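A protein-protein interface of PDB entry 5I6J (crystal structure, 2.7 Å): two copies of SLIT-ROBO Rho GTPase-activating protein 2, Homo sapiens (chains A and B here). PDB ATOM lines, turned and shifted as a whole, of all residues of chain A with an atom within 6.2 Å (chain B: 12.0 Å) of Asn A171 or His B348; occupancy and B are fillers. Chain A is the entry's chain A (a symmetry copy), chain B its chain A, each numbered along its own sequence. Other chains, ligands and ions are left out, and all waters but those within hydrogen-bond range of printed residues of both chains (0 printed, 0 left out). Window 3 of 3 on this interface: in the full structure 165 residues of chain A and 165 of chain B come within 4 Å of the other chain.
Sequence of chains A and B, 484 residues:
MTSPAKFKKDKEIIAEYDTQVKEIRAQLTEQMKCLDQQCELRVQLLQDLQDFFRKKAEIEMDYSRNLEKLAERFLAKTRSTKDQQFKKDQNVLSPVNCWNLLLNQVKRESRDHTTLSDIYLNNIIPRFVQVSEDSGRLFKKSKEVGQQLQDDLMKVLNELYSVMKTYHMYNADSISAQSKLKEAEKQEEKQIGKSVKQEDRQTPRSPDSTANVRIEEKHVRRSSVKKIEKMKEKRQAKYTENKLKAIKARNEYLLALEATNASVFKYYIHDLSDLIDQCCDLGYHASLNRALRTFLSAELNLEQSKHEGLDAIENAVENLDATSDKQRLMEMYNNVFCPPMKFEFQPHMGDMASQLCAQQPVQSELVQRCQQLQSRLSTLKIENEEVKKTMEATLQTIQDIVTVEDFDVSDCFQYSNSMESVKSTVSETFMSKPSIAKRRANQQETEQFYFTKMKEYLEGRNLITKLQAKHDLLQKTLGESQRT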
ATOM      1  N   LYS A   8     -22.338  18.158  -8.019  1.00  0.00           N
ATOM      2  CA  LYS A   8     -21.489  18.362  -6.794  1.00  0.00           C
ATOM      3  C   LYS A   8     -19.965  18.405  -7.074  1.00  0.00           C
ATOM      4  O   LYS A   8     -19.335  17.349  -7.282  1.00  0.00           O
ATOM      5  CB  LYS A   8     -21.834  17.286  -5.755  1.00  0.00           C
ATOM      6  CG  LYS A   8     -22.625  17.776  -4.552  1.00  0.00           C
ATOM      7  CD  LYS A   8     -21.714  17.923  -3.341  1.00  0.00           C
ATOM      8  CE  LYS A   8     -22.414  17.490  -2.062  1.00  0.00           C
ATOM      9  NZ  LYS A   8     -21.448  17.282  -0.944  1.00  0.00           N
ATOM     10  N   LYS A   9     -19.385  19.617  -7.051  1.00  0.00           N
ATOM     11  CA  LYS A   9     -17.981  19.872  -7.481  1.00  0.00           C
ATOM     12  C   LYS A   9     -16.851  19.353  -6.571  1.00  0.00           C
ATOM     13  O   LYS A   9     -17.096  18.980  -5.421  1.00  0.00           O
ATOM     14  CB  LYS A   9     -17.769  21.372  -7.762  1.00  0.00           C
ATOM     15  CG  LYS A   9     -17.655  21.758  -9.239  1.00  0.00           C
ATOM     16  CD  LYS A   9     -19.009  21.965  -9.914  1.00  0.00           C
ATOM     17  CE  LYS A   9     -19.472  20.721 -10.664  1.00  0.00           C
ATOM     18  NZ  LYS A   9     -20.953  20.687 -10.803  1.00  0.00           N
ATOM     19  N   ASP A  10     -15.623  19.342  -7.109  1.00  0.00           N
ATOM     20  CA  ASP A  10     -14.387  18.975  -6.381  1.00  0.00           C
ATOM     21  C   ASP A  10     -14.088  19.872  -5.193  1.00  0.00           C
ATOM     22  O   ASP A  10     -13.833  19.389  -4.089  1.00  0.00           O
ATOM     23  CB  ASP A  10     -13.168  19.040  -7.307  1.00  0.00           C
ATOM     24  CG  ASP A  10     -13.262  18.086  -8.460  1.00  0.00           C
ATOM     25  OD1 ASP A  10     -14.213  18.213  -9.258  1.00  0.00           O
ATOM     26  OD2 ASP A  10     -12.381  17.207  -8.569  1.00  0.00           O
ATOM     27  N   ILE A  13     -16.983  19.629  -2.448  1.00  0.00           N
ATOM     28  CA  ILE A  13     -16.863  18.404  -1.616  1.00  0.00           C
ATOM     29  C   ILE A  13     -15.763  18.582  -0.551  1.00  0.00           C
ATOM     30  O   ILE A  13     -15.949  18.228   0.619  1.00  0.00           O
ATOM     31  CB  ILE A  13     -16.633  17.126  -2.486  1.00  0.00           C
ATOM     32  CG1 ILE A  13     -17.951  16.661  -3.123  1.00  0.00           C
ATOM     33  CG2 ILE A  13     -16.035  15.981  -1.671  1.00  0.00           C
ATOM     34  CD1 ILE A  13     -17.785  15.784  -4.351  1.00  0.00           C
ATOM     35  N   THR A 166      -6.611  12.079  -4.193  1.00  0.00           N
ATOM     36  CA  THR A 166      -6.096  11.044  -5.075  1.00  0.00           C
ATOM     37  C   THR A 166      -7.271  10.423  -5.813  1.00  0.00           C
ATOM     38  O   THR A 166      -7.212  10.241  -7.037  1.00  0.00           O
ATOM     39  CB  THR A 166      -5.330   9.908  -4.342  1.00  0.00           C
ATOM     40  OG1 THR A 166      -4.575  10.423  -3.241  1.00  0.00           O
ATOM     41  CG2 THR A 166      -4.370   9.162  -5.287  1.00  0.00           C
ATOM     42  N   TYR A 167      -8.338  10.107  -5.087  1.00  0.00           N
ATOM     43  CA  TYR A 167      -9.526   9.593  -5.744  1.00  0.00           C
ATOM     44  C   TYR A 167     -10.155  10.616  -6.683  1.00  0.00           C
ATOM     45  O   TYR A 167     -10.538  10.275  -7.794  1.00  0.00           O
ATOM     46  CB  TYR A 167     -10.529   9.071  -4.734  1.00  0.00           C
ATOM     47  CG  TYR A 167     -11.973   8.996  -5.209  1.00  0.00           C
ATOM     48  CD1 TYR A 167     -12.398   8.002  -6.106  1.00  0.00           C
ATOM     49  CD2 TYR A 167     -12.929   9.891  -4.721  1.00  0.00           C
ATOM     50  CE1 TYR A 167     -13.727   7.927  -6.522  1.00  0.00           C
ATOM     51  CE2 TYR A 167     -14.260   9.814  -5.119  1.00  0.00           C
ATOM     52  CZ  TYR A 167     -14.656   8.833  -6.018  1.00  0.00           C
ATOM     53  OH  TYR A 167     -15.976   8.774  -6.399  1.00  0.00           O
ATOM     54  N   HIS A 168     -10.249  11.862  -6.244  1.00  0.00           N
ATOM     55  CA  HIS A 168     -10.820  12.901  -7.083  1.00  0.00           C
ATOM     56  C   HIS A 168     -10.051  13.059  -8.396  1.00  0.00           C
ATOM     57  O   HIS A 168     -10.655  13.287  -9.443  1.00  0.00           O
ATOM     58  CB  HIS A 168     -10.904  14.208  -6.305  1.00  0.00           C
ATOM     59  CG  HIS A 168     -12.090  14.279  -5.400  1.00  0.00           C
ATOM     60  ND1 HIS A 168     -12.686  15.472  -5.050  1.00  0.00           N
ATOM     61  CD2 HIS A 168     -12.813  13.307  -4.795  1.00  0.00           C
ATOM     62  CE1 HIS A 168     -13.717  15.232  -4.257  1.00  0.00           C
ATOM     63  NE2 HIS A 168     -13.815  13.926  -4.084  1.00  0.00           N
ATOM     64  N   MET A 169      -8.734  12.886  -8.331  1.00  0.00           N
ATOM     65  CA  MET A 169      -7.837  13.038  -9.470  1.00  0.00           C
ATOM     66  C   MET A 169      -8.027  11.892 -10.481  1.00  0.00           C
ATOM     67  O   MET A 169      -8.451  12.124 -11.617  1.00  0.00           O
ATOM     68  CB  MET A 169      -6.402  13.105  -8.949  1.00  0.00           C
ATOM     69  CG  MET A 169      -5.396  13.716  -9.895  1.00  0.00           C
ATOM     70  SD  MET A 169      -3.781  13.851  -9.101  1.00  0.00           S
ATOM     71  CE  MET A 169      -3.096  12.190  -9.196  1.00  0.00           C
ATOM     72  N   TYR A 170      -7.743  10.662 -10.042  1.00  0.00           N
ATOM     73  CA  TYR A 170      -7.916   9.440 -10.850  1.00  0.00           C
ATOM     74  C   TYR A 170      -9.349   9.165 -11.273  1.00  0.00           C
ATOM     75  O   TYR A 170      -9.602   8.193 -11.958  1.00  0.00           O
ATOM     76  CB  TYR A 170      -7.366   8.194 -10.132  1.00  0.00           C
ATOM     77  CG  TYR A 170      -5.874   8.192  -9.886  1.00  0.00           C
ATOM     78  CD1 TYR A 170      -5.004   9.008 -10.635  1.00  0.00           C
ATOM     79  CD2 TYR A 170      -5.313   7.352  -8.912  1.00  0.00           C
ATOM     80  CE1 TYR A 170      -3.628   8.997 -10.408  1.00  0.00           C
ATOM     81  CE2 TYR A 170      -3.935   7.328  -8.675  1.00  0.00           C
ATOM     82  CZ  TYR A 170      -3.101   8.156  -9.423  1.00  0.00           C
ATOM     83  OH  TYR A 170      -1.748   8.147  -9.204  1.00  0.00           O
ATOM     84  N   ASN A 171     -10.287  10.000 -10.857  1.00  0.00           N
ATOM     85  CA  ASN A 171     -11.637   9.944 -11.395  1.00  0.00           C
ATOM     86  C   ASN A 171     -11.826  10.969 -12.505  1.00  0.00           C
ATOM     87  O   ASN A 171     -12.663  10.782 -13.390  1.00  0.00           O
ATOM     88  CB  ASN A 171     -12.669  10.184 -10.310  1.00  0.00           C
ATOM     89  CG  ASN A 171     -13.925   9.375 -10.525  1.00  0.00           C
ATOM     90  OD1 ASN A 171     -13.873   8.143 -10.605  1.00  0.00           O
ATOM     91  ND2 ASN A 171     -15.071  10.058 -10.598  1.00  0.00           N
ATOM     92  N   ALA A 172     -11.056  12.056 -12.450  1.00  0.00           N
ATOM     93  CA  ALA A 172     -11.056  13.060 -13.521  1.00  0.00           C
ATOM     94  C   ALA A 172     -10.390  12.487 -14.769  1.00  0.00           C
ATOM     95  O   ALA A 172     -10.811  12.790 -15.887  1.00  0.00           O
ATOM     96  CB  ALA A 172     -10.366  14.344 -13.075  1.00  0.00           C
ATOM     97  N   ASP A 173      -9.365  11.655 -14.553  1.00  0.00           N
ATOM     98  CA  ASP A 173      -8.650  10.939 -15.613  1.00  0.00           C
ATOM     99  C   ASP A 173      -9.509   9.861 -16.260  1.00  0.00           C
ATOM    100  O   ASP A 173      -9.489   9.698 -17.479  1.00  0.00           O
ATOM    101  CB  ASP A 173      -7.359  10.310 -15.068  1.00  0.00           C
ATOM    102  CG  ASP A 173      -6.276  11.345 -14.756  1.00  0.00           C
ATOM    103  OD1 ASP A 173      -6.479  12.561 -14.994  1.00  0.00           O
ATOM    104  OD2 ASP A 173      -5.203  10.927 -14.269  1.00  0.00           O
ATOM    105  N   SER A 174     -10.261   9.134 -15.438  1.00  0.00           N
ATOM    106  CA  SER A 174     -11.126   8.061 -15.918  1.00  0.00           C
ATOM    107  C   SER A 174     -12.449   8.566 -16.524  1.00  0.00           C
ATOM    108  O   SER A 174     -13.177   7.789 -17.156  1.00  0.00           O
ATOM    109  CB  SER A 174     -11.376   7.039 -14.801  1.00  0.00           C
ATOM    110  OG  SER A 174     -12.144   5.932 -15.252  1.00  0.00           O
ATOM    111  N   ILE A 175     -12.759   9.848 -16.325  1.00  0.00           N
ATOM    112  CA  ILE A 175     -13.896  10.485 -17.016  1.00  0.00           C
ATOM    113  C   ILE A 175     -13.428  11.073 -18.375  1.00  0.00           C
ATOM    114  O   ILE A 175     -14.123  10.918 -19.391  1.00  0.00           O
ATOM    115  CB  ILE A 175     -14.696  11.471 -16.083  1.00  0.00           C
ATOM    116  CG1 ILE A 175     -15.626  10.701 -15.086  1.00  0.00           C
ATOM    117  CG2 ILE A 175     -15.427  12.576 -16.863  1.00  0.00           C
ATOM    118  CD1 ILE A 175     -16.976  10.175 -15.583  1.00  0.00           C
ATOM    119  N   SER A 176     -12.238  11.688 -18.387  1.00  0.00           N
ATOM    120  CA  SER A 176     -11.641  12.313 -19.591  1.00  0.00           C
ATOM    121  C   SER A 176     -11.244  11.324 -20.694  1.00  0.00           C
ATOM    122  O   SER A 176     -11.489  11.593 -21.878  1.00  0.00           O
ATOM    123  CB  SER A 176     -10.436  13.180 -19.212  1.00  0.00           C
ATOM    124  OG  SER A 176     -10.215  14.190 -20.177  1.00  0.00           O
ATOM    125  N   ALA A 246      -8.816   4.489 -11.038  1.00  0.00           N
ATOM    126  CA  ALA A 246      -9.978   5.036 -10.317  1.00  0.00           C
ATOM    127  C   ALA A 246     -10.492   4.074  -9.247  1.00  0.00           C
ATOM    128  O   ALA A 246     -10.727   4.487  -8.110  1.00  0.00           O
ATOM    129  CB  ALA A 246     -11.111   5.419 -11.273  1.00  0.00           C
ATOM    130  N   ARG A 250     -10.543   4.691  -5.346  1.00  0.00           N
ATOM    131  CA  ARG A 250     -11.837   4.738  -4.655  1.00  0.00           C
ATOM    132  C   ARG A 250     -11.885   3.738  -3.467  1.00  0.00           C
ATOM    133  O   ARG A 250     -12.470   4.009  -2.400  1.00  0.00           O
ATOM    134  CB  ARG A 250     -12.984   4.493  -5.630  1.00  0.00           C
ATOM    135  CG  ARG A 250     -14.364   4.763  -5.042  1.00  0.00           C
ATOM    136  CD  ARG A 250     -15.469   3.915  -5.681  1.00  0.00           C
ATOM    137  NE  ARG A 250     -15.864   4.425  -6.997  1.00  0.00           N
ATOM    138  CZ  ARG A 250     -15.578   3.838  -8.151  1.00  0.00           C
ATOM    139  NH1 ARG A 250     -14.910   2.691  -8.180  1.00  0.00           N
ATOM    140  NH2 ARG A 250     -15.965   4.403  -9.280  1.00  0.00           N
ATOM    141  N   GLU B 344     -19.311  10.799   5.398  1.00  0.00           N
ATOM    142  CA  GLU B 344     -19.981   9.983   4.404  1.00  0.00           C
ATOM    143  C   GLU B 344     -19.114   9.899   3.154  1.00  0.00           C
ATOM    144  O   GLU B 344     -18.249  10.758   2.937  1.00  0.00           O
ATOM    145  CB  GLU B 344     -21.392  10.517   4.091  1.00  0.00           C
ATOM    146  CG  GLU B 344     -22.364  10.601   5.278  1.00  0.00           C
ATOM    147  CD  GLU B 344     -22.833   9.251   5.842  1.00  0.00           C
ATOM    148  OE1 GLU B 344     -23.670   9.287   6.770  1.00  0.00           O
ATOM    149  OE2 GLU B 344     -22.387   8.159   5.395  1.00  0.00           O
ATOM    150  N   PHE B 345     -19.312   8.835   2.369  1.00  0.00           N
ATOM    151  CA  PHE B 345     -18.744   8.742   1.033  1.00  0.00           C
ATOM    152  C   PHE B 345     -19.290   9.890   0.176  1.00  0.00           C
ATOM    153  O   PHE B 345     -20.509  10.122   0.099  1.00  0.00           O
ATOM    154  CB  PHE B 345     -19.042   7.389   0.392  1.00  0.00           C
ATOM    155  CG  PHE B 345     -18.481   7.249  -0.998  1.00  0.00           C
ATOM    156  CD1 PHE B 345     -17.182   6.765  -1.201  1.00  0.00           C
ATOM    157  CD2 PHE B 345     -19.243   7.616  -2.122  1.00  0.00           C
ATOM    158  CE1 PHE B 345     -16.661   6.647  -2.490  1.00  0.00           C
ATOM    159  CE2 PHE B 345     -18.722   7.504  -3.408  1.00  0.00           C
ATOM    160  CZ  PHE B 345     -17.427   7.023  -3.590  1.00  0.00           C
ATOM    161  N   GLN B 346     -18.375  10.614  -0.451  1.00  0.00           N
ATOM    162  CA  GLN B 346     -18.751  11.772  -1.222  1.00  0.00           C
ATOM    163  C   GLN B 346     -18.396  11.525  -2.690  1.00  0.00           C
ATOM    164  O   GLN B 346     -17.220  11.697  -3.071  1.00  0.00           O
ATOM    165  CB  GLN B 346     -18.098  13.031  -0.630  1.00  0.00           C
ATOM    166  CG  GLN B 346     -19.045  14.220  -0.431  1.00  0.00           C
ATOM    167  CD  GLN B 346     -20.375  13.894   0.265  1.00  0.00           C
ATOM    168  OE1 GLN B 346     -21.437  14.318  -0.190  1.00  0.00           O
ATOM    169  NE2 GLN B 346     -20.320  13.163   1.370  1.00  0.00           N
ATOM    170  N   PRO B 347     -19.412  11.099  -3.510  1.00  0.00           N
ATOM    171  CA  PRO B 347     -19.189  10.696  -4.904  1.00  0.00           C
ATOM    172  C   PRO B 347     -18.809  11.866  -5.792  1.00  0.00           C
ATOM    173  O   PRO B 347     -19.398  12.956  -5.705  1.00  0.00           O
ATOM    174  CB  PRO B 347     -20.528  10.075  -5.320  1.00  0.00           C
ATOM    175  CG  PRO B 347     -21.544  10.720  -4.445  1.00  0.00           C
ATOM    176  CD  PRO B 347     -20.846  10.990  -3.143  1.00  0.00           C
ATOM    177  N   HIS B 348     -17.800  11.618  -6.616  1.00  0.00           N
ATOM    178  CA  HIS B 348     -17.227  12.611  -7.517  1.00  0.00           C
ATOM    179  C   HIS B 348     -17.724  12.417  -8.950  1.00  0.00           C
ATOM    180  O   HIS B 348     -17.648  11.305  -9.504  1.00  0.00           O
ATOM    181  CB  HIS B 348     -15.699  12.544  -7.465  1.00  0.00           C
ATOM    182  CG  HIS B 348     -15.015  13.573  -8.306  1.00  0.00           C
ATOM    183  ND1 HIS B 348     -13.833  13.320  -8.968  1.00  0.00           N
ATOM    184  CD2 HIS B 348     -15.343  14.856  -8.592  1.00  0.00           C
ATOM    185  CE1 HIS B 348     -13.462  14.403  -9.625  1.00  0.00           C
ATOM    186  NE2 HIS B 348     -14.365  15.346  -9.420  1.00  0.00           N
ATOM    187  N   MET B 349     -18.228  13.512  -9.528  1.00  0.00           N
ATOM    188  CA  MET B 349     -18.808  13.544 -10.884  1.00  0.00           C
ATOM    189  C   MET B 349     -20.050  12.640 -11.036  1.00  0.00           C
ATOM    190  O   MET B 349     -20.385  12.212 -12.139  1.00  0.00           O
ATOM    191  CB  MET B 349     -17.743  13.238 -11.966  1.00  0.00           C
ATOM    192  CG  MET B 349     -16.510  14.135 -11.934  1.00  0.00           C
ATOM    193  SD  MET B 349     -16.846  15.857 -12.370  1.00  0.00           S
ATOM    194  CE  MET B 349     -17.025  15.814 -14.163  1.00  0.00           C
ATOM    195  N   GLY B 350     -20.726  12.372  -9.919  1.00  0.00           N
ATOM    196  CA  GLY B 350     -21.948  11.567  -9.887  1.00  0.00           C
ATOM    197  C   GLY B 350     -21.715  10.081 -10.068  1.00  0.00           C
ATOM    198  O   GLY B 350     -22.444   9.436 -10.807  1.00  0.00           O
ATOM    199  N   ASP B 351     -20.700   9.558  -9.382  1.00  0.00           N
ATOM    200  CA  ASP B 351     -20.303   8.147  -9.391  1.00  0.00           C
ATOM    201  C   ASP B 351     -21.461   7.186  -9.088  1.00  0.00           C
ATOM    202  O   ASP B 351     -22.288   7.451  -8.215  1.00  0.00           O
ATOM    203  CB  ASP B 351     -19.184   7.942  -8.364  1.00  0.00           C
ATOM    204  CG  ASP B 351     -18.324   6.707  -8.646  1.00  0.00           C
ATOM    205  OD1 ASP B 351     -18.868   5.592  -8.880  1.00  0.00           O
ATOM    206  OD2 ASP B 351     -17.084   6.861  -8.590  1.00  0.00           O
ATOM    207  N   MET B 352     -21.485   6.067  -9.812  1.00  0.00           N
ATOM    208  CA  MET B 352     -22.619   5.139  -9.810  1.00  0.00           C
ATOM    209  C   MET B 352     -22.538   4.129  -8.656  1.00  0.00           C
ATOM    210  O   MET B 352     -23.515   3.963  -7.916  1.00  0.00           O
ATOM    211  CB  MET B 352     -22.764   4.438 -11.185  1.00  0.00           C
ATOM    212  CG  MET B 352     -23.034   5.369 -12.374  1.00  0.00           C
ATOM    213  SD  MET B 352     -24.770   5.803 -12.666  1.00  0.00           S
ATOM    214  CE  MET B 352     -24.659   7.525 -13.174  1.00  0.00           C
ATOM    215  N   ALA B 353     -21.385   3.462  -8.522  1.00  0.00           N
ATOM    216  CA  ALA B 353     -21.098   2.521  -7.421  1.00  0.00           C
ATOM    217  C   ALA B 353     -20.422   3.260  -6.261  1.00  0.00           C
ATOM    218  O   ALA B 353     -19.881   4.350  -6.452  1.00  0.00           O
ATOM    219  CB  ALA B 353     -20.236   1.360  -7.905  1.00  0.00           C
ATOM    220  N   SER B 354     -20.470   2.679  -5.062  1.00  0.00           N
ATOM    221  CA  SER B 354     -20.012   3.370  -3.853  1.00  0.00           C
ATOM    222  C   SER B 354     -19.711   2.391  -2.721  1.00  0.00           C
ATOM    223  O   SER B 354     -19.893   2.699  -1.541  1.00  0.00           O
ATOM    224  CB  SER B 354     -21.073   4.366  -3.403  1.00  0.00           C
ATOM    225  OG  SER B 354     -22.196   3.665  -2.921  1.00  0.00           O
ATOM    226  N   GLN B 355     -19.259   1.206  -3.105  1.00  0.00           N
ATOM    227  CA  GLN B 355     -18.860   0.145  -2.182  1.00  0.00           C
ATOM    228  C   GLN B 355     -17.458  -0.307  -2.624  1.00  0.00           C
ATOM    229  O   GLN B 355     -16.932   0.182  -3.631  1.00  0.00           O
ATOM    230  CB  GLN B 355     -19.863  -1.033  -2.241  1.00  0.00           C
ATOM    231  CG  GLN B 355     -21.352  -0.664  -2.267  1.00  0.00           C
ATOM    232  CD  GLN B 355     -22.153  -1.465  -3.301  1.00  0.00           C
ATOM    233  OE1 GLN B 355     -22.996  -2.295  -2.941  1.00  0.00           O
ATOM    234  NE2 GLN B 355     -21.891  -1.214  -4.594  1.00  0.00           N
ATOM    235  N   CYS B 357     -15.077  -2.319  -4.649  1.00  0.00           N
ATOM    236  CA  CYS B 357     -15.085  -3.086  -5.886  1.00  0.00           C
ATOM    237  C   CYS B 357     -13.988  -4.162  -5.833  1.00  0.00           C
ATOM    238  O   CYS B 357     -12.800  -3.839  -5.908  1.00  0.00           O
ATOM    239  CB  CYS B 357     -14.911  -2.157  -7.094  1.00  0.00           C
ATOM    240  SG  CYS B 357     -15.378  -2.910  -8.672  1.00  0.00           S
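Of the 13 printed residues of chain B, 5 touch a printed residue of chain A. Printed residues of chain B that touch a printed residue of chain A: Phe B345, Gln B346, Pro B347, His B348 and Asp B351. Hydrophobic or aromatic side chains of chain B that line the printed part of chain A: Phe B345 and His B348. Among the printed residues, 11 pairs touch across the chains. Among the printed residues, Asp or Glu carboxylates within 4 Å of a Lys or Arg side-chain nitrogen of the other chain: Arg A250 with Asp B351 (2.8 Å).
OD2 of Asp B351 lies within salt-bridge range of NH2 of Arg A250, 2.8 Å away. NE2 of His B348 sits at hydrogen-bond distance from OD2 of Asp A10 (2.9 Å). The side-chain amide oxygen (OE1) of Gln B346 lies within hydrogen-bond range of the side-chain amino group (NZ) of Lys A8 (3.1 Å). ND1 of His B348 lies close to O of His A168 (3.2 Å). OH of Tyr A167 lies within hydrogen-bond range of N of His B348, at 3.4 Å. O of His B348 lies within hydrogen-bond range of ND2 of Asn A171 (3.1 Å). The side-chain hydroxyl of Tyr A167 is in hydrogen-bond range of the side-chain carboxylate of Asp B351, 3.1 Å away.
Ile A13 touches Gln B346. Ile A13 touches Pro B347. Tyr A167 touches Phe B345. Arg A250 touches Phe B345.
No position is printed for both chains.
OD1 of Asp B351 is in hydrogen-bond range of N of Ala B353, at 3.3 Å.
Of the printed residues of chain B, Asn A171 touches His B348. His B348 touches just these residues of chain A: Asp A10, Tyr A167, His A168 and Asn A171. Tyr A167 touches just these residues of chain B: Phe B345, His B348 and Asp B351. Met A169 touches none of the printed residues of chain B. No residue of chain B comes within 4 Å of Asp A173. No residue of chain B comes within 4 Å of Ser A174. Printed residues of chain A within 4 Å of Pro B347: Ile A13 (3.5 Å). Of the printed residues of chain A, Asp B351 touches Tyr A167 (3.1 Å) and Arg A250 (2.8 Å). Ser B354 touches none of the printed residues of chain A. The nearest residue of chain A that does not touch His B348 is Ala A172 (4.4 Å). The nearest printed residue of chain B that does not touch Ile A13 is His B348 (4.5 Å).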
